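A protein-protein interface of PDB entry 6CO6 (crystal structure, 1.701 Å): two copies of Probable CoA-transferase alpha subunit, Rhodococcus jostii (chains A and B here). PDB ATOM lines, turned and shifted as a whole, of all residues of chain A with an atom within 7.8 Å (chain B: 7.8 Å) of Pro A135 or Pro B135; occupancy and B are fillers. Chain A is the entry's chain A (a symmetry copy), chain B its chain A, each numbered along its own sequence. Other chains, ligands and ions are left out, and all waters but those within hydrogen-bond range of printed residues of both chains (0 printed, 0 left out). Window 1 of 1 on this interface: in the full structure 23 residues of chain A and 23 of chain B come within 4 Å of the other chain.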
ATOM      1  N   CYS A 122      20.839 -28.892 -15.413  1.00  0.00           N
ATOM      2  CA  CYS A 122      19.661 -29.080 -14.574  1.00  0.00           C
ATOM      3  C   CYS A 122      19.416 -30.559 -14.277  1.00  0.00           C
ATOM      4  O   CYS A 122      19.173 -30.944 -13.126  1.00  0.00           O
ATOM      5  CB  CYS A 122      18.467 -28.433 -15.275  1.00  0.00           C
ATOM      6  SG  CYS A 122      16.886 -28.612 -14.456  1.00  0.00           S
ATOM      7  N   ALA A 126      19.462 -32.393 -10.643  1.00  0.00           N
ATOM      8  CA  ALA A 126      18.370 -33.182 -10.082  1.00  0.00           C
ATOM      9  C   ALA A 126      18.894 -34.513  -9.564  1.00  0.00           C
ATOM     10  O   ALA A 126      18.603 -34.907  -8.433  1.00  0.00           O
ATOM     11  CB  ALA A 126      17.264 -33.388 -11.121  1.00  0.00           C
ATOM     12  N   ALA A 129      20.852 -34.223  -6.318  1.00  0.00           N
ATOM     13  CA  ALA A 129      19.976 -34.018  -5.169  1.00  0.00           C
ATOM     14  C   ALA A 129      19.013 -35.181  -4.946  1.00  0.00           C
ATOM     15  O   ALA A 129      18.122 -35.087  -4.088  1.00  0.00           O
ATOM     16  CB  ALA A 129      19.180 -32.722  -5.347  1.00  0.00           C
ATOM     17  N   LEU A 131      16.581 -36.001  -6.674  1.00  0.00           N
ATOM     18  CA  LEU A 131      15.246 -35.568  -7.055  1.00  0.00           C
ATOM     19  C   LEU A 131      14.843 -36.185  -8.386  1.00  0.00           C
ATOM     20  O   LEU A 131      15.685 -36.379  -9.263  1.00  0.00           O
ATOM     21  CB  LEU A 131      15.192 -34.044  -7.177  1.00  0.00           C
ATOM     22  CG  LEU A 131      15.375 -33.314  -5.846  1.00  0.00           C
ATOM     23  CD1 LEU A 131      15.616 -31.840  -6.110  1.00  0.00           C
ATOM     24  CD2 LEU A 131      14.152 -33.510  -4.946  1.00  0.00           C
ATOM     25  N   PRO A 132      13.557 -36.482  -8.587  1.00  0.00           N
ATOM     26  CA  PRO A 132      13.140 -37.046  -9.877  1.00  0.00           C
ATOM     27  C   PRO A 132      13.080 -36.035 -11.001  1.00  0.00           C
ATOM     28  O   PRO A 132      13.110 -36.445 -12.171  1.00  0.00           O
ATOM     29  CB  PRO A 132      11.744 -37.622  -9.580  1.00  0.00           C
ATOM     30  CG  PRO A 132      11.245 -36.805  -8.412  1.00  0.00           C
ATOM     31  CD  PRO A 132      12.454 -36.436  -7.608  1.00  0.00           C
ATOM     32  N   PHE A 133      13.003 -34.740 -10.699  1.00  0.00           N
ATOM     33  CA  PHE A 133      12.954 -33.715 -11.734  1.00  0.00           C
ATOM     34  C   PHE A 133      13.333 -32.387 -11.106  1.00  0.00           C
ATOM     35  O   PHE A 133      13.303 -32.232  -9.885  1.00  0.00           O
ATOM     36  CB  PHE A 133      11.559 -33.591 -12.363  1.00  0.00           C
ATOM     37  CG  PHE A 133      10.567 -32.888 -11.468  1.00  0.00           C
ATOM     38  CD1 PHE A 133       9.901 -33.585 -10.467  1.00  0.00           C
ATOM     39  CD2 PHE A 133      10.334 -31.526 -11.601  1.00  0.00           C
ATOM     40  CE1 PHE A 133       9.008 -32.942  -9.614  1.00  0.00           C
ATOM     41  CE2 PHE A 133       9.445 -30.870 -10.742  1.00  0.00           C
ATOM     42  CZ  PHE A 133       8.782 -31.581  -9.753  1.00  0.00           C
ATOM     43  N   LEU A 134      13.674 -31.433 -11.962  1.00  0.00           N
ATOM     44  CA  LEU A 134      13.670 -30.026 -11.597  1.00  0.00           C
ATOM     45  C   LEU A 134      12.962 -29.258 -12.699  1.00  0.00           C
ATOM     46  O   LEU A 134      13.129 -29.582 -13.881  1.00  0.00           O
ATOM     47  CB  LEU A 134      15.089 -29.467 -11.420  1.00  0.00           C
ATOM     48  CG  LEU A 134      15.863 -29.931 -10.193  1.00  0.00           C
ATOM     49  CD1 LEU A 134      17.314 -29.538 -10.349  1.00  0.00           C
ATOM     50  CD2 LEU A 134      15.260 -29.314  -8.905  1.00  0.00           C
ATOM     51  N   PRO A 135      12.176 -28.245 -12.349  1.00  0.00           N
ATOM     52  CA  PRO A 135      11.504 -27.436 -13.368  1.00  0.00           C
ATOM     53  C   PRO A 135      12.481 -26.493 -14.049  1.00  0.00           C
ATOM     54  O   PRO A 135      13.438 -26.008 -13.442  1.00  0.00           O
ATOM     55  CB  PRO A 135      10.472 -26.647 -12.556  1.00  0.00           C
ATOM     56  CG  PRO A 135      11.166 -26.459 -11.227  1.00  0.00           C
ATOM     57  CD  PRO A 135      11.943 -27.727 -10.985  1.00  0.00           C
ATOM     58  N   ILE A 136      12.211 -26.208 -15.321  1.00  0.00           N
ATOM     59  CA  ILE A 136      13.070 -25.320 -16.100  1.00  0.00           C
ATOM     60  C   ILE A 136      12.246 -24.789 -17.262  1.00  0.00           C
ATOM     61  O   ILE A 136      11.342 -25.468 -17.757  1.00  0.00           O
ATOM     62  CB  ILE A 136      14.351 -26.063 -16.569  1.00  0.00           C
ATOM     63  CG1 ILE A 136      15.374 -25.094 -17.176  1.00  0.00           C
ATOM     64  CG2 ILE A 136      14.011 -27.222 -17.544  1.00  0.00           C
ATOM     65  CD1 ILE A 136      16.786 -25.676 -17.323  1.00  0.00           C
ATOM     66  N   ARG A 137      12.531 -23.542 -17.674  1.00  0.00           N
ATOM     67  CA  ARG A 137      11.856 -22.976 -18.842  1.00  0.00           C
ATOM     68  C   ARG A 137      12.433 -23.525 -20.143  1.00  0.00           C
ATOM     69  O   ARG A 137      11.682 -23.823 -21.085  1.00  0.00           O
ATOM     70  CB  ARG A 137      11.958 -21.447 -18.829  1.00  0.00           C
ATOM     71  CG  ARG A 137      10.741 -20.721 -18.258  1.00  0.00           C
ATOM     72  CD  ARG A 137      11.002 -19.209 -18.168  1.00  0.00           C
ATOM     73  NE  ARG A 137      12.354 -18.987 -17.688  1.00  0.00           N
ATOM     74  CZ  ARG A 137      12.686 -18.880 -16.406  1.00  0.00           C
ATOM     75  NH1 ARG A 137      11.747 -18.935 -15.467  1.00  0.00           N
ATOM     76  NH2 ARG A 137      13.955 -18.715 -16.069  1.00  0.00           N
ATOM     77  N   ALA A 138      13.756 -23.661 -20.217  1.00  0.00           N
ATOM     78  CA  ALA A 138      14.413 -24.122 -21.434  1.00  0.00           C
ATOM     79  C   ALA A 138      13.792 -25.418 -21.933  1.00  0.00           C
ATOM     80  O   ALA A 138      13.583 -26.360 -21.164  1.00  0.00           O
ATOM     81  CB  ALA A 138      15.910 -24.324 -21.178  1.00  0.00           C
ATOM     82  N   THR A 154       5.857 -32.059 -18.655  1.00  0.00           N
ATOM     83  CA  THR A 154       5.810 -30.769 -17.980  1.00  0.00           C
ATOM     84  C   THR A 154       5.353 -30.932 -16.536  1.00  0.00           C
ATOM     85  O   THR A 154       4.879 -31.993 -16.112  1.00  0.00           O
ATOM     86  CB  THR A 154       4.878 -29.796 -18.716  1.00  0.00           C
ATOM     87  OG1 THR A 154       3.550 -30.344 -18.766  1.00  0.00           O
ATOM     88  CG2 THR A 154       5.376 -29.537 -20.134  1.00  0.00           C
ATOM     89  N   VAL A 155       5.497 -29.845 -15.774  1.00  0.00           N
ATOM     90  CA  VAL A 155       4.995 -29.775 -14.411  1.00  0.00           C
ATOM     91  C   VAL A 155       4.388 -28.393 -14.212  1.00  0.00           C
ATOM     92  O   VAL A 155       4.944 -27.384 -14.660  1.00  0.00           O
ATOM     93  CB  VAL A 155       6.107 -30.075 -13.379  1.00  0.00           C
ATOM     94  CG1 VAL A 155       7.271 -29.091 -13.514  1.00  0.00           C
ATOM     95  CG2 VAL A 155       5.538 -30.063 -11.960  1.00  0.00           C
ATOM     96  N   THR A 156       3.233 -28.341 -13.568  1.00  0.00           N
ATOM     97  CA  THR A 156       2.572 -27.066 -13.322  1.00  0.00           C
ATOM     98  C   THR A 156       2.829 -26.611 -11.894  1.00  0.00           C
ATOM     99  O   THR A 156       2.736 -27.409 -10.954  1.00  0.00           O
ATOM    100  CB  THR A 156       1.074 -27.168 -13.583  1.00  0.00           C
ATOM    101  OG1 THR A 156       0.865 -27.539 -14.947  1.00  0.00           O
ATOM    102  CG2 THR A 156       0.397 -25.810 -13.327  1.00  0.00           C
ATOM    103  N   SER A 157       3.163 -25.338 -11.743  1.00  0.00           N
ATOM    104  CA  SER A 157       3.376 -24.764 -10.424  1.00  0.00           C
ATOM    105  C   SER A 157       2.115 -24.893  -9.575  1.00  0.00           C
ATOM    106  O   SER A 157       1.019 -24.573 -10.052  1.00  0.00           O
ATOM    107  CB  SER A 157       3.748 -23.289 -10.558  1.00  0.00           C
ATOM    108  OG  SER A 157       3.873 -22.677  -9.289  1.00  0.00           O
ATOM    109  N   THR A 168       3.382 -23.502 -16.393  1.00  0.00           N
ATOM    110  CA  THR A 168       3.673 -24.893 -16.693  1.00  0.00           C
ATOM    111  C   THR A 168       5.042 -24.937 -17.356  1.00  0.00           C
ATOM    112  O   THR A 168       5.277 -24.257 -18.361  1.00  0.00           O
ATOM    113  CB  THR A 168       2.580 -25.499 -17.567  1.00  0.00           C
ATOM    114  OG1 THR A 168       1.378 -25.580 -16.787  1.00  0.00           O
ATOM    115  CG2 THR A 168       2.967 -26.899 -18.020  1.00  0.00           C
ATOM    116  N   LEU A 169       5.954 -25.679 -16.742  1.00  0.00           N
ATOM    117  CA  LEU A 169       7.366 -25.680 -17.089  1.00  0.00           C
ATOM    118  C   LEU A 169       7.789 -27.079 -17.504  1.00  0.00           C
ATOM    119  O   LEU A 169       7.108 -28.059 -17.201  1.00  0.00           O
ATOM    120  CB  LEU A 169       8.207 -25.219 -15.889  1.00  0.00           C
ATOM    121  CG  LEU A 169       7.869 -23.801 -15.447  1.00  0.00           C
ATOM    122  CD1 LEU A 169       8.018 -23.613 -13.939  1.00  0.00           C
ATOM    123  CD2 LEU A 169       8.753 -22.865 -16.236  1.00  0.00           C
ATOM    124  N   ILE A 170       8.937 -27.172 -18.186  1.00  0.00           N
ATOM    125  CA  ILE A 170       9.545 -28.480 -18.419  1.00  0.00           C
ATOM    126  C   ILE A 170       9.917 -29.107 -17.084  1.00  0.00           C
ATOM    127  O   ILE A 170      10.555 -28.470 -16.233  1.00  0.00           O
ATOM    128  CB  ILE A 170      10.791 -28.361 -19.311  1.00  0.00           C
ATOM    129  CG1 ILE A 170      10.457 -27.721 -20.660  1.00  0.00           C
ATOM    130  CG2 ILE A 170      11.429 -29.733 -19.520  1.00  0.00           C
ATOM    131  CD1 ILE A 170       9.563 -28.550 -21.520  1.00  0.00           C
ATOM    132  N   ALA A 171       9.547 -30.373 -16.901  1.00  0.00           N
ATOM    133  CA  ALA A 171      10.033 -31.138 -15.757  1.00  0.00           C
ATOM    134  C   ALA A 171      11.265 -31.872 -16.254  1.00  0.00           C
ATOM    135  O   ALA A 171      11.168 -32.940 -16.858  1.00  0.00           O
ATOM    136  CB  ALA A 171       8.964 -32.096 -15.238  1.00  0.00           C
ATOM    137  N   MET A 172      12.438 -31.271 -16.060  1.00  0.00           N
ATOM    138  CA  MET A 172      13.661 -31.925 -16.534  1.00  0.00           C
ATOM    139  C   MET A 172      13.926 -33.147 -15.673  1.00  0.00           C
ATOM    140  O   MET A 172      14.142 -32.999 -14.466  1.00  0.00           O
ATOM    141  CB  MET A 172      14.853 -30.974 -16.472  1.00  0.00           C
ATOM    142  CG  MET A 172      16.163 -31.637 -16.872  1.00  0.00           C
ATOM    143  SD  MET A 172      16.156 -32.147 -18.598  1.00  0.00           S
ATOM    144  CE  MET A 172      17.510 -33.333 -18.617  1.00  0.00           C
ATOM    145  N   PRO A 173      13.929 -34.356 -16.223  1.00  0.00           N
ATOM    146  CA  PRO A 173      14.164 -35.535 -15.383  1.00  0.00           C
ATOM    147  C   PRO A 173      15.614 -35.611 -14.935  1.00  0.00           C
ATOM    148  O   PRO A 173      16.524 -35.077 -15.570  1.00  0.00           O
ATOM    149  CB  PRO A 173      13.808 -36.704 -16.303  1.00  0.00           C
ATOM    150  CG  PRO A 173      14.156 -36.181 -17.672  1.00  0.00           C
ATOM    151  CD  PRO A 173      13.719 -34.721 -17.639  1.00  0.00           C
ATOM    152  N   CYS B 122      17.101 -22.831  -1.303  1.00  0.00           N
ATOM    153  CA  CYS B 122      16.257 -23.276  -2.406  1.00  0.00           C
ATOM    154  C   CYS B 122      15.301 -22.175  -2.858  1.00  0.00           C
ATOM    155  O   CYS B 122      15.160 -21.909  -4.060  1.00  0.00           O
ATOM    156  CB  CYS B 122      15.509 -24.532  -1.957  1.00  0.00           C
ATOM    157  SG  CYS B 122      14.346 -25.214  -3.133  1.00  0.00           S
ATOM    158  N   ALA B 126      15.155 -20.371  -6.506  1.00  0.00           N
ATOM    159  CA  ALA B 126      13.977 -20.294  -7.362  1.00  0.00           C
ATOM    160  C   ALA B 126      13.765 -18.865  -7.839  1.00  0.00           C
ATOM    161  O   ALA B 126      13.577 -18.621  -9.034  1.00  0.00           O
ATOM    162  CB  ALA B 126      12.740 -20.822  -6.629  1.00  0.00           C
ATOM    163  N   ALA B 129      16.240 -17.766 -10.508  1.00  0.00           N
ATOM    164  CA  ALA B 129      15.928 -18.343 -11.812  1.00  0.00           C
ATOM    165  C   ALA B 129      14.563 -17.910 -12.338  1.00  0.00           C
ATOM    166  O   ALA B 129      14.109 -18.425 -13.372  1.00  0.00           O
ATOM    167  CB  ALA B 129      15.984 -19.871 -11.731  1.00  0.00           C
ATOM    168  N   LEU B 131      11.769 -18.727 -11.291  1.00  0.00           N
ATOM    169  CA  LEU B 131      10.864 -19.862 -11.202  1.00  0.00           C
ATOM    170  C   LEU B 131       9.886 -19.678 -10.051  1.00  0.00           C
ATOM    171  O   LEU B 131      10.240 -19.110  -9.018  1.00  0.00           O
ATOM    172  CB  LEU B 131      11.649 -21.157 -10.985  1.00  0.00           C
ATOM    173  CG  LEU B 131      12.516 -21.559 -12.179  1.00  0.00           C
ATOM    174  CD1 LEU B 131      13.474 -22.656 -11.759  1.00  0.00           C
ATOM    175  CD2 LEU B 131      11.645 -22.019 -13.351  1.00  0.00           C
ATOM    176  N   PRO B 132       8.652 -20.171 -10.178  1.00  0.00           N
ATOM    177  CA  PRO B 132       7.703 -20.035  -9.066  1.00  0.00           C
ATOM    178  C   PRO B 132       7.961 -20.984  -7.916  1.00  0.00           C
ATOM    179  O   PRO B 132       7.481 -20.716  -6.805  1.00  0.00           O
ATOM    180  CB  PRO B 132       6.341 -20.324  -9.722  1.00  0.00           C
ATOM    181  CG  PRO B 132       6.677 -21.192 -10.912  1.00  0.00           C
ATOM    182  CD  PRO B 132       8.032 -20.758 -11.381  1.00  0.00           C
ATOM    183  N   PHE B 133       8.698 -22.073  -8.132  1.00  0.00           N
ATOM    184  CA  PHE B 133       8.994 -23.020  -7.065  1.00  0.00           C
ATOM    185  C   PHE B 133      10.188 -23.855  -7.489  1.00  0.00           C
ATOM    186  O   PHE B 133      10.536 -23.910  -8.668  1.00  0.00           O
ATOM    187  CB  PHE B 133       7.809 -23.953  -6.772  1.00  0.00           C
ATOM    188  CG  PHE B 133       7.627 -25.024  -7.820  1.00  0.00           C
ATOM    189  CD1 PHE B 133       6.941 -24.751  -8.998  1.00  0.00           C
ATOM    190  CD2 PHE B 133       8.177 -26.286  -7.646  1.00  0.00           C
ATOM    191  CE1 PHE B 133       6.793 -25.720  -9.986  1.00  0.00           C
ATOM    192  CE2 PHE B 133       8.040 -27.264  -8.638  1.00  0.00           C
ATOM    193  CZ  PHE B 133       7.346 -26.978  -9.804  1.00  0.00           C
ATOM    194  N   LEU B 134      10.795 -24.513  -6.509  1.00  0.00           N
ATOM    195  CA  LEU B 134      11.668 -25.647  -6.761  1.00  0.00           C
ATOM    196  C   LEU B 134      11.280 -26.758  -5.801  1.00  0.00           C
ATOM    197  O   LEU B 134      10.954 -26.484  -4.640  1.00  0.00           O
ATOM    198  CB  LEU B 134      13.149 -25.297  -6.560  1.00  0.00           C
ATOM    199  CG  LEU B 134      13.789 -24.390  -7.603  1.00  0.00           C
ATOM    200  CD1 LEU B 134      15.124 -23.909  -7.084  1.00  0.00           C
ATOM    201  CD2 LEU B 134      13.958 -25.143  -8.947  1.00  0.00           C
ATOM    202  N   PRO B 135      11.308 -28.009  -6.250  1.00  0.00           N
ATOM    203  CA  PRO B 135      10.991 -29.128  -5.360  1.00  0.00           C
ATOM    204  C   PRO B 135      12.137 -29.406  -4.402  1.00  0.00           C
ATOM    205  O   PRO B 135      13.311 -29.223  -4.732  1.00  0.00           O
ATOM    206  CB  PRO B 135      10.805 -30.298  -6.330  1.00  0.00           C
ATOM    207  CG  PRO B 135      11.772 -29.966  -7.443  1.00  0.00           C
ATOM    208  CD  PRO B 135      11.732 -28.467  -7.589  1.00  0.00           C
ATOM    209  N   ILE B 136      11.785 -29.885  -3.212  1.00  0.00           N
ATOM    210  CA  ILE B 136      12.785 -30.190  -2.190  1.00  0.00           C
ATOM    211  C   ILE B 136      12.158 -31.177  -1.217  1.00  0.00           C
ATOM    212  O   ILE B 136      10.943 -31.162  -0.999  1.00  0.00           O
ATOM    213  CB  ILE B 136      13.274 -28.893  -1.491  1.00  0.00           C
ATOM    214  CG1 ILE B 136      14.488 -29.161  -0.592  1.00  0.00           C
ATOM    215  CG2 ILE B 136      12.125 -28.201  -0.710  1.00  0.00           C
ATOM    216  CD1 ILE B 136      15.248 -27.899  -0.162  1.00  0.00           C
ATOM    217  N   ARG B 137      12.988 -32.074  -0.660  1.00  0.00           N
ATOM    218  CA  ARG B 137      12.498 -33.005   0.356  1.00  0.00           C
ATOM    219  C   ARG B 137      12.344 -32.323   1.713  1.00  0.00           C
ATOM    220  O   ARG B 137      11.360 -32.569   2.428  1.00  0.00           O
ATOM    221  CB  ARG B 137      13.442 -34.207   0.480  1.00  0.00           C
ATOM    222  CG  ARG B 137      13.018 -35.447  -0.305  1.00  0.00           C
ATOM    223  CD  ARG B 137      14.096 -36.539  -0.220  1.00  0.00           C
ATOM    224  NE  ARG B 137      15.405 -35.927  -0.354  1.00  0.00           N
ATOM    225  CZ  ARG B 137      16.028 -35.734  -1.511  1.00  0.00           C
ATOM    226  NH1 ARG B 137      15.472 -36.148  -2.645  1.00  0.00           N
ATOM    227  NH2 ARG B 137      17.206 -35.133  -1.529  1.00  0.00           N
ATOM    228  N   ALA B 138      13.299 -31.473   2.083  1.00  0.00           N
ATOM    229  CA  ALA B 138      13.278 -30.813   3.383  1.00  0.00           C
ATOM    230  C   ALA B 138      11.940 -30.132   3.627  1.00  0.00           C
ATOM    231  O   ALA B 138      11.424 -29.416   2.764  1.00  0.00           O
ATOM    232  CB  ALA B 138      14.411 -29.787   3.469  1.00  0.00           C
ATOM    233  N   THR B 154       2.677 -28.880  -1.891  1.00  0.00           N
ATOM    234  CA  THR B 154       3.522 -29.920  -2.462  1.00  0.00           C
ATOM    235  C   THR B 154       3.406 -29.937  -3.982  1.00  0.00           C
ATOM    236  O   THR B 154       2.532 -29.298  -4.580  1.00  0.00           O
ATOM    237  CB  THR B 154       3.158 -31.300  -1.895  1.00  0.00           C
ATOM    238  OG1 THR B 154       1.785 -31.598  -2.198  1.00  0.00           O
ATOM    239  CG2 THR B 154       3.368 -31.337  -0.385  1.00  0.00           C
ATOM    240  N   VAL B 155       4.309 -30.696  -4.606  1.00  0.00           N
ATOM    241  CA  VAL B 155       4.269 -30.936  -6.040  1.00  0.00           C
ATOM    242  C   VAL B 155       4.610 -32.400  -6.274  1.00  0.00           C
ATOM    243  O   VAL B 155       5.513 -32.952  -5.636  1.00  0.00           O
ATOM    244  CB  VAL B 155       5.223 -29.989  -6.803  1.00  0.00           C
ATOM    245  CG1 VAL B 155       6.669 -30.155  -6.328  1.00  0.00           C
ATOM    246  CG2 VAL B 155       5.110 -30.214  -8.311  1.00  0.00           C
ATOM    247  N   THR B 156       3.873 -33.046  -7.164  1.00  0.00           N
ATOM    248  CA  THR B 156       4.123 -34.450  -7.464  1.00  0.00           C
ATOM    249  C   THR B 156       4.916 -34.575  -8.756  1.00  0.00           C
ATOM    250  O   THR B 156       4.614 -33.902  -9.747  1.00  0.00           O
ATOM    251  CB  THR B 156       2.817 -35.227  -7.568  1.00  0.00           C
ATOM    252  OG1 THR B 156       2.123 -35.138  -6.321  1.00  0.00           O
ATOM    253  CG2 THR B 156       3.102 -36.707  -7.876  1.00  0.00           C
ATOM    254  N   SER B 157       5.932 -35.425  -8.730  1.00  0.00           N
ATOM    255  CA  SER B 157       6.732 -35.682  -9.917  1.00  0.00           C
ATOM    256  C   SER B 157       5.857 -36.222 -11.044  1.00  0.00           C
ATOM    257  O   SER B 157       5.056 -37.137 -10.814  1.00  0.00           O
ATOM    258  CB  SER B 157       7.825 -36.698  -9.593  1.00  0.00           C
ATOM    259  OG  SER B 157       8.564 -37.039 -10.749  1.00  0.00           O
ATOM    260  N   THR B 168       6.052 -37.155  -4.036  1.00  0.00           N
ATOM    261  CA  THR B 168       5.430 -35.869  -3.780  1.00  0.00           C
ATOM    262  C   THR B 168       6.337 -35.110  -2.820  1.00  0.00           C
ATOM    263  O   THR B 168       6.671 -35.613  -1.740  1.00  0.00           O
ATOM    264  CB  THR B 168       4.018 -36.047  -3.231  1.00  0.00           C
ATOM    265  OG1 THR B 168       3.202 -36.599  -4.275  1.00  0.00           O
ATOM    266  CG2 THR B 168       3.433 -34.709  -2.804  1.00  0.00           C
ATOM    267  N   LEU B 169       6.787 -33.942  -3.257  1.00  0.00           N
ATOM    268  CA  LEU B 169       7.826 -33.173  -2.590  1.00  0.00           C
ATOM    269  C   LEU B 169       7.278 -31.813  -2.192  1.00  0.00           C
ATOM    270  O   LEU B 169       6.258 -31.366  -2.716  1.00  0.00           O
ATOM    271  CB  LEU B 169       9.033 -32.992  -3.523  1.00  0.00           C
ATOM    272  CG  LEU B 169       9.664 -34.318  -3.927  1.00  0.00           C
ATOM    273  CD1 LEU B 169      10.241 -34.279  -5.341  1.00  0.00           C
ATOM    274  CD2 LEU B 169      10.708 -34.650  -2.887  1.00  0.00           C
ATOM    275  N   ILE B 170       7.977 -31.141  -1.268  1.00  0.00           N
ATOM    276  CA  ILE B 170       7.670 -29.739  -0.996  1.00  0.00           C
ATOM    277  C   ILE B 170       7.924 -28.916  -2.250  1.00  0.00           C
ATOM    278  O   ILE B 170       8.988 -29.019  -2.879  1.00  0.00           O
ATOM    279  CB  ILE B 170       8.517 -29.202   0.168  1.00  0.00           C
ATOM    280  CG1 ILE B 170       8.296 -30.015   1.445  1.00  0.00           C
ATOM    281  CG2 ILE B 170       8.204 -27.728   0.419  1.00  0.00           C
ATOM    282  CD1 ILE B 170       6.920 -29.898   2.009  1.00  0.00           C
ATOM    283  N   ALA B 171       6.962 -28.068  -2.606  1.00  0.00           N
ATOM    284  CA  ALA B 171       7.185 -27.079  -3.659  1.00  0.00           C
ATOM    285  C   ALA B 171       7.633 -25.819  -2.943  1.00  0.00           C
ATOM    286  O   ALA B 171       6.815 -25.038  -2.458  1.00  0.00           O
ATOM    287  CB  ALA B 171       5.920 -26.854  -4.482  1.00  0.00           C
ATOM    288  N   MET B 172       8.948 -25.641  -2.813  1.00  0.00           N
ATOM    289  CA  MET B 172       9.439 -24.449  -2.115  1.00  0.00           C
ATOM    290  C   MET B 172       9.164 -23.230  -2.977  1.00  0.00           C
ATOM    291  O   MET B 172       9.700 -23.143  -4.087  1.00  0.00           O
ATOM    292  CB  MET B 172      10.934 -24.557  -1.827  1.00  0.00           C
ATOM    293  CG  MET B 172      11.507 -23.304  -1.181  1.00  0.00           C
ATOM    294  SD  MET B 172      10.812 -23.015   0.453  1.00  0.00           S
ATOM    295  CE  MET B 172      11.215 -21.279   0.701  1.00  0.00           C
ATOM    296  N   PRO B 173       8.358 -22.273  -2.532  1.00  0.00           N
ATOM    297  CA  PRO B 173       8.079 -21.108  -3.378  1.00  0.00           C
ATOM    298  C   PRO B 173       9.291 -20.197  -3.479  1.00  0.00           C
ATOM    299  O   PRO B 173      10.165 -20.172  -2.611  1.00  0.00           O
ATOM    300  CB  PRO B 173       6.923 -20.412  -2.654  1.00  0.00           C
ATOM    301  CG  PRO B 173       7.174 -20.748  -1.208  1.00  0.00           C
ATOM    302  CD  PRO B 173       7.656 -22.194  -1.235  1.00  0.00           C
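The backbone NH (N) of Met A172 lies within hydrogen-bond range of the backbone carbonyl oxygen (O) of Leu A134, 2.8 Å away.
O of Ala A126 lies within hydrogen-bond range of N of Leu A131, at 2.9 Å.
N of Val B155 lies within hydrogen-bond range of O of Leu B169 (2.8 Å).
N of Leu B131 sits at hydrogen-bond distance from O of Ala B126 (2.9 Å).
N of Val A155 is in hydrogen-bond range of O of Leu A169 (2.8 Å).
The backbone carbonyl oxygen (O) of Leu B134 sits at hydrogen-bond distance from the backbone NH (N) of Met B172.
CD1 of Leu A131 touches O of Pro B135 (3.7 Å).
Arg B137 touches Leu A131 (NH1 to CD2, 3.7 Å).
Pro A132 touches Leu B169.
CE1 of Phe A133 touches CA of Ser B157, at 3.6 Å.
CG of Pro A135 touches O of Phe B133, 3.7 Å away.
Pro A135 touches Leu B134.
Pro A135 touches Pro B135 (CD to CD, 3.5 Å).
Arg A137 touches Leu B131 (NH1 to CD2, 3.7 Å).
Ser A157 touches Pro B132.
Pro B132 touches Leu A169.
NH2 of Arg B137 lies within hydrogen-bond range of O of Ala A129, 2.7 Å away.
The guanidinium group (NH2) of Arg A137 sits at hydrogen-bond distance from the backbone carbonyl oxygen (O) of Ala B129 (2.7 Å).
Ala A129 touches Arg B137, and with the chains exchanged Arg A137 touches Ala B129.
Leu A131 touches Pro B135, and with the chains exchanged Pro A135 touches Leu B131.
Phe A133 touches Pro B135, and with the chains exchanged Pro A135 touches Phe B133.
Phe A133 touches Ser B157, and with the chains exchanged Ser A157 touches Phe B133.
Positions printed for both chains: 122, 126, 129, 131, 132, 133, 134, 135, 136, 137, 138, 154, 155, 156, 157, 168, 169, 170, 171, 172 and 173.
Hydrophobic or aromatic side chains of chain A that line the printed part of chain B: Leu A131, Pro A132, Phe A133, Leu A134, Pro A135, Val A155 and Leu A169.
Along chain B the printed residues that touch a printed residue of chain A span positions 129 to 169.
Of the printed residues of chain B, Val A155 touches Val B155.
Of the printed residues of chain B, Leu A134 touches Pro B135.
The nearest printed residue of chain A that does not touch Pro B132 is Arg A137 (5.8 Å).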
